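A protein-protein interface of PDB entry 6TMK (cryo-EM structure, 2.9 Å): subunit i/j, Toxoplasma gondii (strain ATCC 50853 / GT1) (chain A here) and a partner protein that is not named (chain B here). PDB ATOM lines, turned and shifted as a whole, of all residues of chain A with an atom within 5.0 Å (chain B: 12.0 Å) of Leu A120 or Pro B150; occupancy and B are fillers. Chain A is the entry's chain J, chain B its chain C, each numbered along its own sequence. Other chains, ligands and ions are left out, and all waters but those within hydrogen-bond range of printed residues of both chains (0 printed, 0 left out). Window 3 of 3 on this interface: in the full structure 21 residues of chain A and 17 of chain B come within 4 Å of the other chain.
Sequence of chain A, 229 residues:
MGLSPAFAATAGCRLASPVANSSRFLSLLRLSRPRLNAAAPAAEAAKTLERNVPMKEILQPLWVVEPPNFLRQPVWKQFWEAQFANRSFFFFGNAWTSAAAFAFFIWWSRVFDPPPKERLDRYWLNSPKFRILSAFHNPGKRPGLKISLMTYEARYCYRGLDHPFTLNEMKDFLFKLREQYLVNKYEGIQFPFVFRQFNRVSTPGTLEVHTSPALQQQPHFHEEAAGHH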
ATOM      1  N   PRO A 115      32.079  15.367  -3.153  1.00  0.00           N
ATOM      2  CA  PRO A 115      31.479  16.683  -3.116  1.00  0.00           C
ATOM      3  C   PRO A 115      30.203  16.671  -2.299  1.00  0.00           C
ATOM      4  O   PRO A 115      29.623  15.604  -2.047  1.00  0.00           O
ATOM      5  CB  PRO A 115      31.195  16.969  -4.594  1.00  0.00           C
ATOM      6  CG  PRO A 115      30.924  15.655  -5.149  1.00  0.00           C
ATOM      7  CD  PRO A 115      31.833  14.703  -4.442  1.00  0.00           C
ATOM      8  N   PRO A 116      29.731  17.830  -1.874  1.00  0.00           N
ATOM      9  CA  PRO A 116      28.433  17.900  -1.211  1.00  0.00           C
ATOM     10  C   PRO A 116      27.254  17.893  -2.179  1.00  0.00           C
ATOM     11  O   PRO A 116      27.376  18.009  -3.411  1.00  0.00           O
ATOM     12  CB  PRO A 116      28.532  19.209  -0.429  1.00  0.00           C
ATOM     13  CG  PRO A 116      29.459  20.034  -1.197  1.00  0.00           C
ATOM     14  CD  PRO A 116      30.480  19.086  -1.732  1.00  0.00           C
ATOM     15  N   LYS A 117      26.074  17.785  -1.568  1.00  0.00           N
ATOM     16  CA  LYS A 117      24.852  17.710  -2.345  1.00  0.00           C
ATOM     17  C   LYS A 117      24.609  19.010  -3.087  1.00  0.00           C
ATOM     18  O   LYS A 117      23.987  19.009  -4.154  1.00  0.00           O
ATOM     19  CB  LYS A 117      23.685  17.369  -1.429  1.00  0.00           C
ATOM     20  CG  LYS A 117      23.848  16.071  -0.688  1.00  0.00           C
ATOM     21  CD  LYS A 117      22.565  15.651  -0.022  1.00  0.00           C
ATOM     22  CE  LYS A 117      22.717  14.376   0.762  1.00  0.00           C
ATOM     23  NZ  LYS A 117      21.396  13.796   1.082  1.00  0.00           N
ATOM     24  N   GLU A 118      25.110  20.120  -2.552  1.00  0.00           N
ATOM     25  CA  GLU A 118      24.985  21.384  -3.251  1.00  0.00           C
ATOM     26  C   GLU A 118      25.789  21.368  -4.538  1.00  0.00           C
ATOM     27  O   GLU A 118      25.511  22.160  -5.442  1.00  0.00           O
ATOM     28  CB  GLU A 118      25.426  22.526  -2.340  1.00  0.00           C
ATOM     29  CG  GLU A 118      26.819  22.382  -1.779  1.00  0.00           C
ATOM     30  CD  GLU A 118      27.301  23.630  -1.068  1.00  0.00           C
ATOM     31  OE1 GLU A 118      26.907  23.842   0.099  1.00  0.00           O
ATOM     32  OE2 GLU A 118      28.080  24.396  -1.672  1.00  0.00           O
ATOM     33  N   ARG A 119      26.781  20.482  -4.636  1.00  0.00           N
ATOM     34  CA  ARG A 119      27.753  20.518  -5.714  1.00  0.00           C
ATOM     35  C   ARG A 119      27.800  19.201  -6.478  1.00  0.00           C
ATOM     36  O   ARG A 119      28.801  18.905  -7.135  1.00  0.00           O
ATOM     37  CB  ARG A 119      29.133  20.857  -5.164  1.00  0.00           C
ATOM     38  CG  ARG A 119      29.980  21.657  -6.101  1.00  0.00           C
ATOM     39  CD  ARG A 119      31.420  21.632  -5.667  1.00  0.00           C
ATOM     40  NE  ARG A 119      31.582  22.127  -4.305  1.00  0.00           N
ATOM     41  CZ  ARG A 119      32.547  21.739  -3.483  1.00  0.00           C
ATOM     42  NH1 ARG A 119      33.448  20.857  -3.870  1.00  0.00           N
ATOM     43  NH2 ARG A 119      32.611  22.236  -2.265  1.00  0.00           N
ATOM     44  N   LEU A 120      26.725  18.414  -6.434  1.00  0.00           N
ATOM     45  CA  LEU A 120      26.758  17.110  -7.089  1.00  0.00           C
ATOM     46  C   LEU A 120      26.517  17.221  -8.592  1.00  0.00           C
ATOM     47  O   LEU A 120      27.105  16.469  -9.377  1.00  0.00           O
ATOM     48  CB  LEU A 120      25.708  16.180  -6.494  1.00  0.00           C
ATOM     49  CG  LEU A 120      25.951  15.537  -5.141  1.00  0.00           C
ATOM     50  CD1 LEU A 120      24.668  14.898  -4.695  1.00  0.00           C
ATOM     51  CD2 LEU A 120      27.056  14.531  -5.206  1.00  0.00           C
ATOM     52  N   ASP A 121      25.661  18.147  -9.009  1.00  0.00           N
ATOM     53  CA  ASP A 121      25.345  18.346 -10.416  1.00  0.00           C
ATOM     54  C   ASP A 121      26.396  19.158 -11.151  1.00  0.00           C
ATOM     55  O   ASP A 121      26.173  19.532 -12.306  1.00  0.00           O
ATOM     56  CB  ASP A 121      23.983  19.020 -10.557  1.00  0.00           C
ATOM     57  CG  ASP A 121      23.972  20.422 -10.011  1.00  0.00           C
ATOM     58  OD1 ASP A 121      24.297  20.601  -8.819  1.00  0.00           O
ATOM     59  OD2 ASP A 121      23.650  21.357 -10.770  1.00  0.00           O
ATOM     60  N   ARG A 122      27.526  19.441 -10.511  1.00  0.00           N
ATOM     61  CA  ARG A 122      28.633  20.091 -11.192  1.00  0.00           C
ATOM     62  C   ARG A 122      29.427  19.089 -12.021  1.00  0.00           C
ATOM     63  O   ARG A 122      29.761  19.357 -13.178  1.00  0.00           O
ATOM     64  CB  ARG A 122      29.536  20.783 -10.172  1.00  0.00           C
ATOM     65  CG  ARG A 122      30.402  21.871 -10.745  1.00  0.00           C
ATOM     66  CD  ARG A 122      29.642  23.160 -10.922  1.00  0.00           C
ATOM     67  NE  ARG A 122      30.385  24.134 -11.712  1.00  0.00           N
ATOM     68  CZ  ARG A 122      31.306  24.954 -11.228  1.00  0.00           C
ATOM     69  NH1 ARG A 122      31.617  24.941  -9.944  1.00  0.00           N
ATOM     70  NH2 ARG A 122      31.914  25.797 -12.036  1.00  0.00           N
ATOM     71  N   TYR A 123      29.747  17.947 -11.441  1.00  0.00           N
ATOM     72  CA  TYR A 123      30.449  16.887 -12.152  1.00  0.00           C
ATOM     73  C   TYR A 123      29.816  15.514 -11.995  1.00  0.00           C
ATOM     74  O   TYR A 123      29.752  14.767 -12.969  1.00  0.00           O
ATOM     75  CB  TYR A 123      31.901  16.844 -11.680  1.00  0.00           C
ATOM     76  CG  TYR A 123      32.814  16.008 -12.530  1.00  0.00           C
ATOM     77  CD1 TYR A 123      33.621  16.597 -13.477  1.00  0.00           C
ATOM     78  CD2 TYR A 123      32.885  14.635 -12.377  1.00  0.00           C
ATOM     79  CE1 TYR A 123      34.461  15.854 -14.251  1.00  0.00           C
ATOM     80  CE2 TYR A 123      33.717  13.885 -13.151  1.00  0.00           C
ATOM     81  CZ  TYR A 123      34.506  14.493 -14.086  1.00  0.00           C
ATOM     82  OH  TYR A 123      35.344  13.732 -14.859  1.00  0.00           O
ATOM     83  N   TRP A 124      29.319  15.172 -10.805  1.00  0.00           N
ATOM     84  CA  TRP A 124      29.119  13.766 -10.472  1.00  0.00           C
ATOM     85  C   TRP A 124      27.931  13.179 -11.217  1.00  0.00           C
ATOM     86  O   TRP A 124      27.983  12.028 -11.663  1.00  0.00           O
ATOM     87  CB  TRP A 124      28.924  13.595  -8.969  1.00  0.00           C
ATOM     88  CG  TRP A 124      28.576  12.203  -8.562  1.00  0.00           C
ATOM     89  CD1 TRP A 124      27.432  11.798  -7.957  1.00  0.00           C
ATOM     90  CD2 TRP A 124      29.371  11.025  -8.733  1.00  0.00           C
ATOM     91  NE1 TRP A 124      27.457  10.454  -7.742  1.00  0.00           N
ATOM     92  CE2 TRP A 124      28.640   9.954  -8.207  1.00  0.00           C
ATOM     93  CE3 TRP A 124      30.628  10.775  -9.279  1.00  0.00           C
ATOM     94  CZ2 TRP A 124      29.115   8.661  -8.212  1.00  0.00           C
ATOM     95  CZ3 TRP A 124      31.096   9.490  -9.277  1.00  0.00           C
ATOM     96  CH2 TRP A 124      30.346   8.450  -8.751  1.00  0.00           C
ATOM     97  N   LEU A 125      26.856  13.943 -11.368  1.00  0.00           N
ATOM     98  CA  LEU A 125      25.665  13.417 -12.012  1.00  0.00           C
ATOM     99  C   LEU A 125      25.805  13.306 -13.521  1.00  0.00           C
ATOM    100  O   LEU A 125      24.900  12.778 -14.172  1.00  0.00           O
ATOM    101  CB  LEU A 125      24.470  14.297 -11.658  1.00  0.00           C
ATOM    102  CG  LEU A 125      24.234  14.474 -10.160  1.00  0.00           C
ATOM    103  CD1 LEU A 125      23.084  15.399  -9.908  1.00  0.00           C
ATOM    104  CD2 LEU A 125      23.974  13.147  -9.504  1.00  0.00           C
ATOM    105  N   PHE A 130      29.197   7.241 -12.352  1.00  0.00           N
ATOM    106  CA  PHE A 130      27.845   7.358 -11.828  1.00  0.00           C
ATOM    107  C   PHE A 130      26.834   6.708 -12.759  1.00  0.00           C
ATOM    108  O   PHE A 130      25.956   5.957 -12.317  1.00  0.00           O
ATOM    109  CB  PHE A 130      27.516   8.830 -11.604  1.00  0.00           C
ATOM    110  CG  PHE A 130      26.078   9.099 -11.349  1.00  0.00           C
ATOM    111  CD1 PHE A 130      25.311   9.718 -12.304  1.00  0.00           C
ATOM    112  CD2 PHE A 130      25.489   8.748 -10.161  1.00  0.00           C
ATOM    113  CE1 PHE A 130      24.002   9.970 -12.080  1.00  0.00           C
ATOM    114  CE2 PHE A 130      24.173   9.004  -9.941  1.00  0.00           C
ATOM    115  CZ  PHE A 130      23.428   9.615 -10.900  1.00  0.00           C
ATOM    116  N   MET A 150      17.207  13.745  -9.733  1.00  0.00           N
ATOM    117  CA  MET A 150      18.260  13.959  -8.749  1.00  0.00           C
ATOM    118  C   MET A 150      18.940  15.301  -8.970  1.00  0.00           C
ATOM    119  O   MET A 150      19.318  15.976  -8.011  1.00  0.00           O
ATOM    120  CB  MET A 150      19.292  12.839  -8.825  1.00  0.00           C
ATOM    121  CG  MET A 150      18.830  11.527  -8.262  1.00  0.00           C
ATOM    122  SD  MET A 150      19.853  10.137  -8.763  1.00  0.00           S
ATOM    123  CE  MET A 150      21.243  10.376  -7.666  1.00  0.00           C
ATOM    124  N   ALA A 154      19.161  18.241  -6.282  1.00  0.00           N
ATOM    125  CA  ALA A 154      20.420  18.820  -5.846  1.00  0.00           C
ATOM    126  C   ALA A 154      20.429  20.326  -6.039  1.00  0.00           C
ATOM    127  O   ALA A 154      21.089  21.042  -5.280  1.00  0.00           O
ATOM    128  CB  ALA A 154      21.577  18.180  -6.605  1.00  0.00           C
ATOM    129  N   ASP B 143      36.836   3.382   1.420  1.00  0.00           N
ATOM    130  CA  ASP B 143      35.814   3.195   0.403  1.00  0.00           C
ATOM    131  C   ASP B 143      34.403   3.309   0.958  1.00  0.00           C
ATOM    132  O   ASP B 143      33.536   3.908   0.314  1.00  0.00           O
ATOM    133  CB  ASP B 143      35.991   1.832  -0.265  1.00  0.00           C
ATOM    134  CG  ASP B 143      37.264   1.737  -1.076  1.00  0.00           C
ATOM    135  OD1 ASP B 143      37.776   0.612  -1.237  1.00  0.00           O
ATOM    136  OD2 ASP B 143      37.758   2.779  -1.550  1.00  0.00           O
ATOM    137  N   TYR B 144      34.145   2.748   2.138  1.00  0.00           N
ATOM    138  CA  TYR B 144      32.793   2.633   2.660  1.00  0.00           C
ATOM    139  C   TYR B 144      32.512   3.587   3.811  1.00  0.00           C
ATOM    140  O   TYR B 144      31.438   3.511   4.412  1.00  0.00           O
ATOM    141  CB  TYR B 144      32.531   1.189   3.081  1.00  0.00           C
ATOM    142  CG  TYR B 144      32.647   0.239   1.922  1.00  0.00           C
ATOM    143  CD1 TYR B 144      31.612   0.085   1.022  1.00  0.00           C
ATOM    144  CD2 TYR B 144      33.801  -0.488   1.715  1.00  0.00           C
ATOM    145  CE1 TYR B 144      31.721  -0.766  -0.039  1.00  0.00           C
ATOM    146  CE2 TYR B 144      33.921  -1.339   0.658  1.00  0.00           C
ATOM    147  CZ  TYR B 144      32.877  -1.478  -0.220  1.00  0.00           C
ATOM    148  OH  TYR B 144      32.997  -2.334  -1.285  1.00  0.00           O
ATOM    149  N   PHE B 145      33.440   4.484   4.134  1.00  0.00           N
ATOM    150  CA  PHE B 145      33.163   5.534   5.101  1.00  0.00           C
ATOM    151  C   PHE B 145      33.534   6.911   4.571  1.00  0.00           C
ATOM    152  O   PHE B 145      32.877   7.901   4.898  1.00  0.00           O
ATOM    153  CB  PHE B 145      33.892   5.245   6.409  1.00  0.00           C
ATOM    154  CG  PHE B 145      33.307   4.110   7.172  1.00  0.00           C
ATOM    155  CD1 PHE B 145      32.303   4.329   8.085  1.00  0.00           C
ATOM    156  CD2 PHE B 145      33.749   2.823   6.971  1.00  0.00           C
ATOM    157  CE1 PHE B 145      31.759   3.287   8.785  1.00  0.00           C
ATOM    158  CE2 PHE B 145      33.209   1.786   7.665  1.00  0.00           C
ATOM    159  CZ  PHE B 145      32.213   2.014   8.574  1.00  0.00           C
ATOM    160  N   TYR B 146      34.576   6.984   3.747  1.00  0.00           N
ATOM    161  CA  TYR B 146      35.125   8.255   3.305  1.00  0.00           C
ATOM    162  C   TYR B 146      34.854   8.581   1.844  1.00  0.00           C
ATOM    163  O   TYR B 146      34.948   9.753   1.471  1.00  0.00           O
ATOM    164  CB  TYR B 146      36.641   8.286   3.536  1.00  0.00           C
ATOM    165  CG  TYR B 146      37.059   8.531   4.961  1.00  0.00           C
ATOM    166  CD1 TYR B 146      37.123   9.812   5.470  1.00  0.00           C
ATOM    167  CD2 TYR B 146      37.402   7.484   5.797  1.00  0.00           C
ATOM    168  CE1 TYR B 146      37.503  10.044   6.763  1.00  0.00           C
ATOM    169  CE2 TYR B 146      37.783   7.710   7.092  1.00  0.00           C
ATOM    170  CZ  TYR B 146      37.835   8.993   7.570  1.00  0.00           C
ATOM    171  OH  TYR B 146      38.218   9.226   8.866  1.00  0.00           O
ATOM    172  N   GLN B 147      34.521   7.596   1.013  1.00  0.00           N
ATOM    173  CA  GLN B 147      34.349   7.803  -0.420  1.00  0.00           C
ATOM    174  C   GLN B 147      33.000   7.295  -0.896  1.00  0.00           C
ATOM    175  O   GLN B 147      32.879   6.718  -1.977  1.00  0.00           O
ATOM    176  CB  GLN B 147      35.469   7.134  -1.207  1.00  0.00           C
ATOM    177  CG  GLN B 147      36.798   7.800  -1.081  1.00  0.00           C
ATOM    178  CD  GLN B 147      36.885   9.089  -1.856  1.00  0.00           C
ATOM    179  OE1 GLN B 147      36.406   9.185  -2.982  1.00  0.00           O
ATOM    180  NE2 GLN B 147      37.508  10.088  -1.262  1.00  0.00           N
ATOM    181  N   ARG B 148      31.964   7.508  -0.101  1.00  0.00           N
ATOM    182  CA  ARG B 148      30.614   7.182  -0.524  1.00  0.00           C
ATOM    183  C   ARG B 148      30.033   8.281  -1.398  1.00  0.00           C
ATOM    184  O   ARG B 148      30.207   9.470  -1.123  1.00  0.00           O
ATOM    185  CB  ARG B 148      29.722   6.972   0.690  1.00  0.00           C
ATOM    186  CG  ARG B 148      30.164   5.866   1.585  1.00  0.00           C
ATOM    187  CD  ARG B 148      29.092   5.545   2.581  1.00  0.00           C
ATOM    188  NE  ARG B 148      28.027   4.748   1.991  1.00  0.00           N
ATOM    189  CZ  ARG B 148      28.066   3.431   1.865  1.00  0.00           C
ATOM    190  NH1 ARG B 148      29.109   2.752   2.287  1.00  0.00           N
ATOM    191  NH2 ARG B 148      27.059   2.790   1.310  1.00  0.00           N
ATOM    192  N   ARG B 149      29.331   7.875  -2.448  1.00  0.00           N
ATOM    193  CA  ARG B 149      28.730   8.800  -3.387  1.00  0.00           C
ATOM    194  C   ARG B 149      27.349   8.287  -3.758  1.00  0.00           C
ATOM    195  O   ARG B 149      27.095   7.080  -3.693  1.00  0.00           O
ATOM    196  CB  ARG B 149      29.586   8.948  -4.650  1.00  0.00           C
ATOM    197  CG  ARG B 149      30.686   9.948  -4.525  1.00  0.00           C
ATOM    198  CD  ARG B 149      31.680   9.785  -5.621  1.00  0.00           C
ATOM    199  NE  ARG B 149      32.796  10.709  -5.501  1.00  0.00           N
ATOM    200  CZ  ARG B 149      33.905  10.449  -4.821  1.00  0.00           C
ATOM    201  NH1 ARG B 149      34.054   9.299  -4.195  1.00  0.00           N
ATOM    202  NH2 ARG B 149      34.866  11.344  -4.759  1.00  0.00           N
ATOM    203  N   PRO B 150      26.444   9.172  -4.161  1.00  0.00           N
ATOM    204  CA  PRO B 150      25.069   8.750  -4.416  1.00  0.00           C
ATOM    205  C   PRO B 150      24.902   8.034  -5.745  1.00  0.00           C
ATOM    206  O   PRO B 150      25.660   8.229  -6.696  1.00  0.00           O
ATOM    207  CB  PRO B 150      24.289  10.068  -4.383  1.00  0.00           C
ATOM    208  CG  PRO B 150      25.259  11.083  -4.711  1.00  0.00           C
ATOM    209  CD  PRO B 150      26.560  10.636  -4.152  1.00  0.00           C
ATOM    210  N   VAL B 151      23.866   7.204  -5.794  1.00  0.00           N
ATOM    211  CA  VAL B 151      23.540   6.387  -6.950  1.00  0.00           C
ATOM    212  C   VAL B 151      22.034   6.431  -7.144  1.00  0.00           C
ATOM    213  O   VAL B 151      21.266   6.523  -6.183  1.00  0.00           O
ATOM    214  CB  VAL B 151      24.047   4.936  -6.783  1.00  0.00           C
ATOM    215  CG1 VAL B 151      23.470   4.028  -7.843  1.00  0.00           C
ATOM    216  CG2 VAL B 151      25.542   4.902  -6.852  1.00  0.00           C
ATOM    217  N   ALA B 152      21.615   6.377  -8.400  1.00  0.00           N
ATOM    218  CA  ALA B 152      20.204   6.473  -8.716  1.00  0.00           C
ATOM    219  C   ALA B 152      19.493   5.149  -8.460  1.00  0.00           C
ATOM    220  O   ALA B 152      20.094   4.075  -8.454  1.00  0.00           O
ATOM    221  CB  ALA B 152      20.008   6.894 -10.172  1.00  0.00           C
ATOM    222  N   TRP B 153      18.183   5.254  -8.254  1.00  0.00           N
ATOM    223  CA  TRP B 153      17.303   4.129  -7.978  1.00  0.00           C
ATOM    224  C   TRP B 153      16.075   4.232  -8.864  1.00  0.00           C
ATOM    225  O   TRP B 153      15.410   5.272  -8.892  1.00  0.00           O
ATOM    226  CB  TRP B 153      16.901   4.100  -6.511  1.00  0.00           C
ATOM    227  CG  TRP B 153      16.442   2.776  -6.018  1.00  0.00           C
ATOM    228  CD1 TRP B 153      15.636   1.894  -6.661  1.00  0.00           C
ATOM    229  CD2 TRP B 153      16.764   2.181  -4.765  1.00  0.00           C
ATOM    230  NE1 TRP B 153      15.431   0.788  -5.885  1.00  0.00           N
ATOM    231  CE2 TRP B 153      16.118   0.938  -4.714  1.00  0.00           C
ATOM    232  CE3 TRP B 153      17.541   2.580  -3.679  1.00  0.00           C
ATOM    233  CZ2 TRP B 153      16.223   0.094  -3.622  1.00  0.00           C
ATOM    234  CZ3 TRP B 153      17.641   1.746  -2.606  1.00  0.00           C
ATOM    235  CH2 TRP B 153      16.988   0.517  -2.579  1.00  0.00           C
ATOM    236  N   CYS B 154      15.771   3.149  -9.567  1.00  0.00           N
ATOM    237  CA  CYS B 154      14.554   3.061 -10.353  1.00  0.00           C
ATOM    238  C   CYS B 154      13.723   1.849  -9.947  1.00  0.00           C
ATOM    239  O   CYS B 154      12.835   1.419 -10.686  1.00  0.00           O
ATOM    240  CB  CYS B 154      14.897   2.971 -11.831  1.00  0.00           C
ATOM    241  SG  CYS B 154      16.045   4.224 -12.393  1.00  0.00           S
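The side-chain amide oxygen (OE1) of Gln B147 sits at hydrogen-bond distance from the guanidinium group (NH1) of Arg B149 (2.6 Å). The backbone carbonyl oxygen of Leu A120 is in hydrogen-bond range of the backbone NH of Leu A125.
Among the printed residues, merely in contact across the chains: Leu A120 with Pro B150 (3.9 Å), Trp A124 with Arg B149 (3.6 Å), Phe A130 with Pro B150 (3.5 Å), Phe A130 with Ala B152 (3.98 Å) and Met A150 with Ala B152 (3.5 Å).
Pro B150 touches just these residues of chain A: Leu A120, Trp A124 and Phe A130. No residue of chain B comes within 4 Å of Pro A115. No residue of chain B comes within 4 Å of Pro A116. Lys A117 touches none of the printed residues of chain B. No residue of chain B comes within 4 Å of Asp A121. Trp A124 touches two residues of chain B. No residue of chain B comes within 4 Å of Leu A125. Phe A130 touches just these residues of chain B: Pro B150 (3.5 Å) and Ala B152 (3.98 Å). Of the printed residues of chain A, Ala B152 touches Phe A130 and Met A150. Of the printed residues of chain B, Met A150 touches Ala B152 (3.5 Å). Of the printed residues of chain A, Arg B149 touches Trp A124.
Along chain A the printed residues that touch a printed residue of chain B span positions 120 to 150. Hydrophobic or aromatic side chains of chain B within 4 Å of the printed part of chain A: Pro B150 and Ala B152. Among the printed residues, 6 pairs touch across the chains.
O of Pro B150 lies within hydrogen-bond range of NE1 of Trp A124 (3.0 Å).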
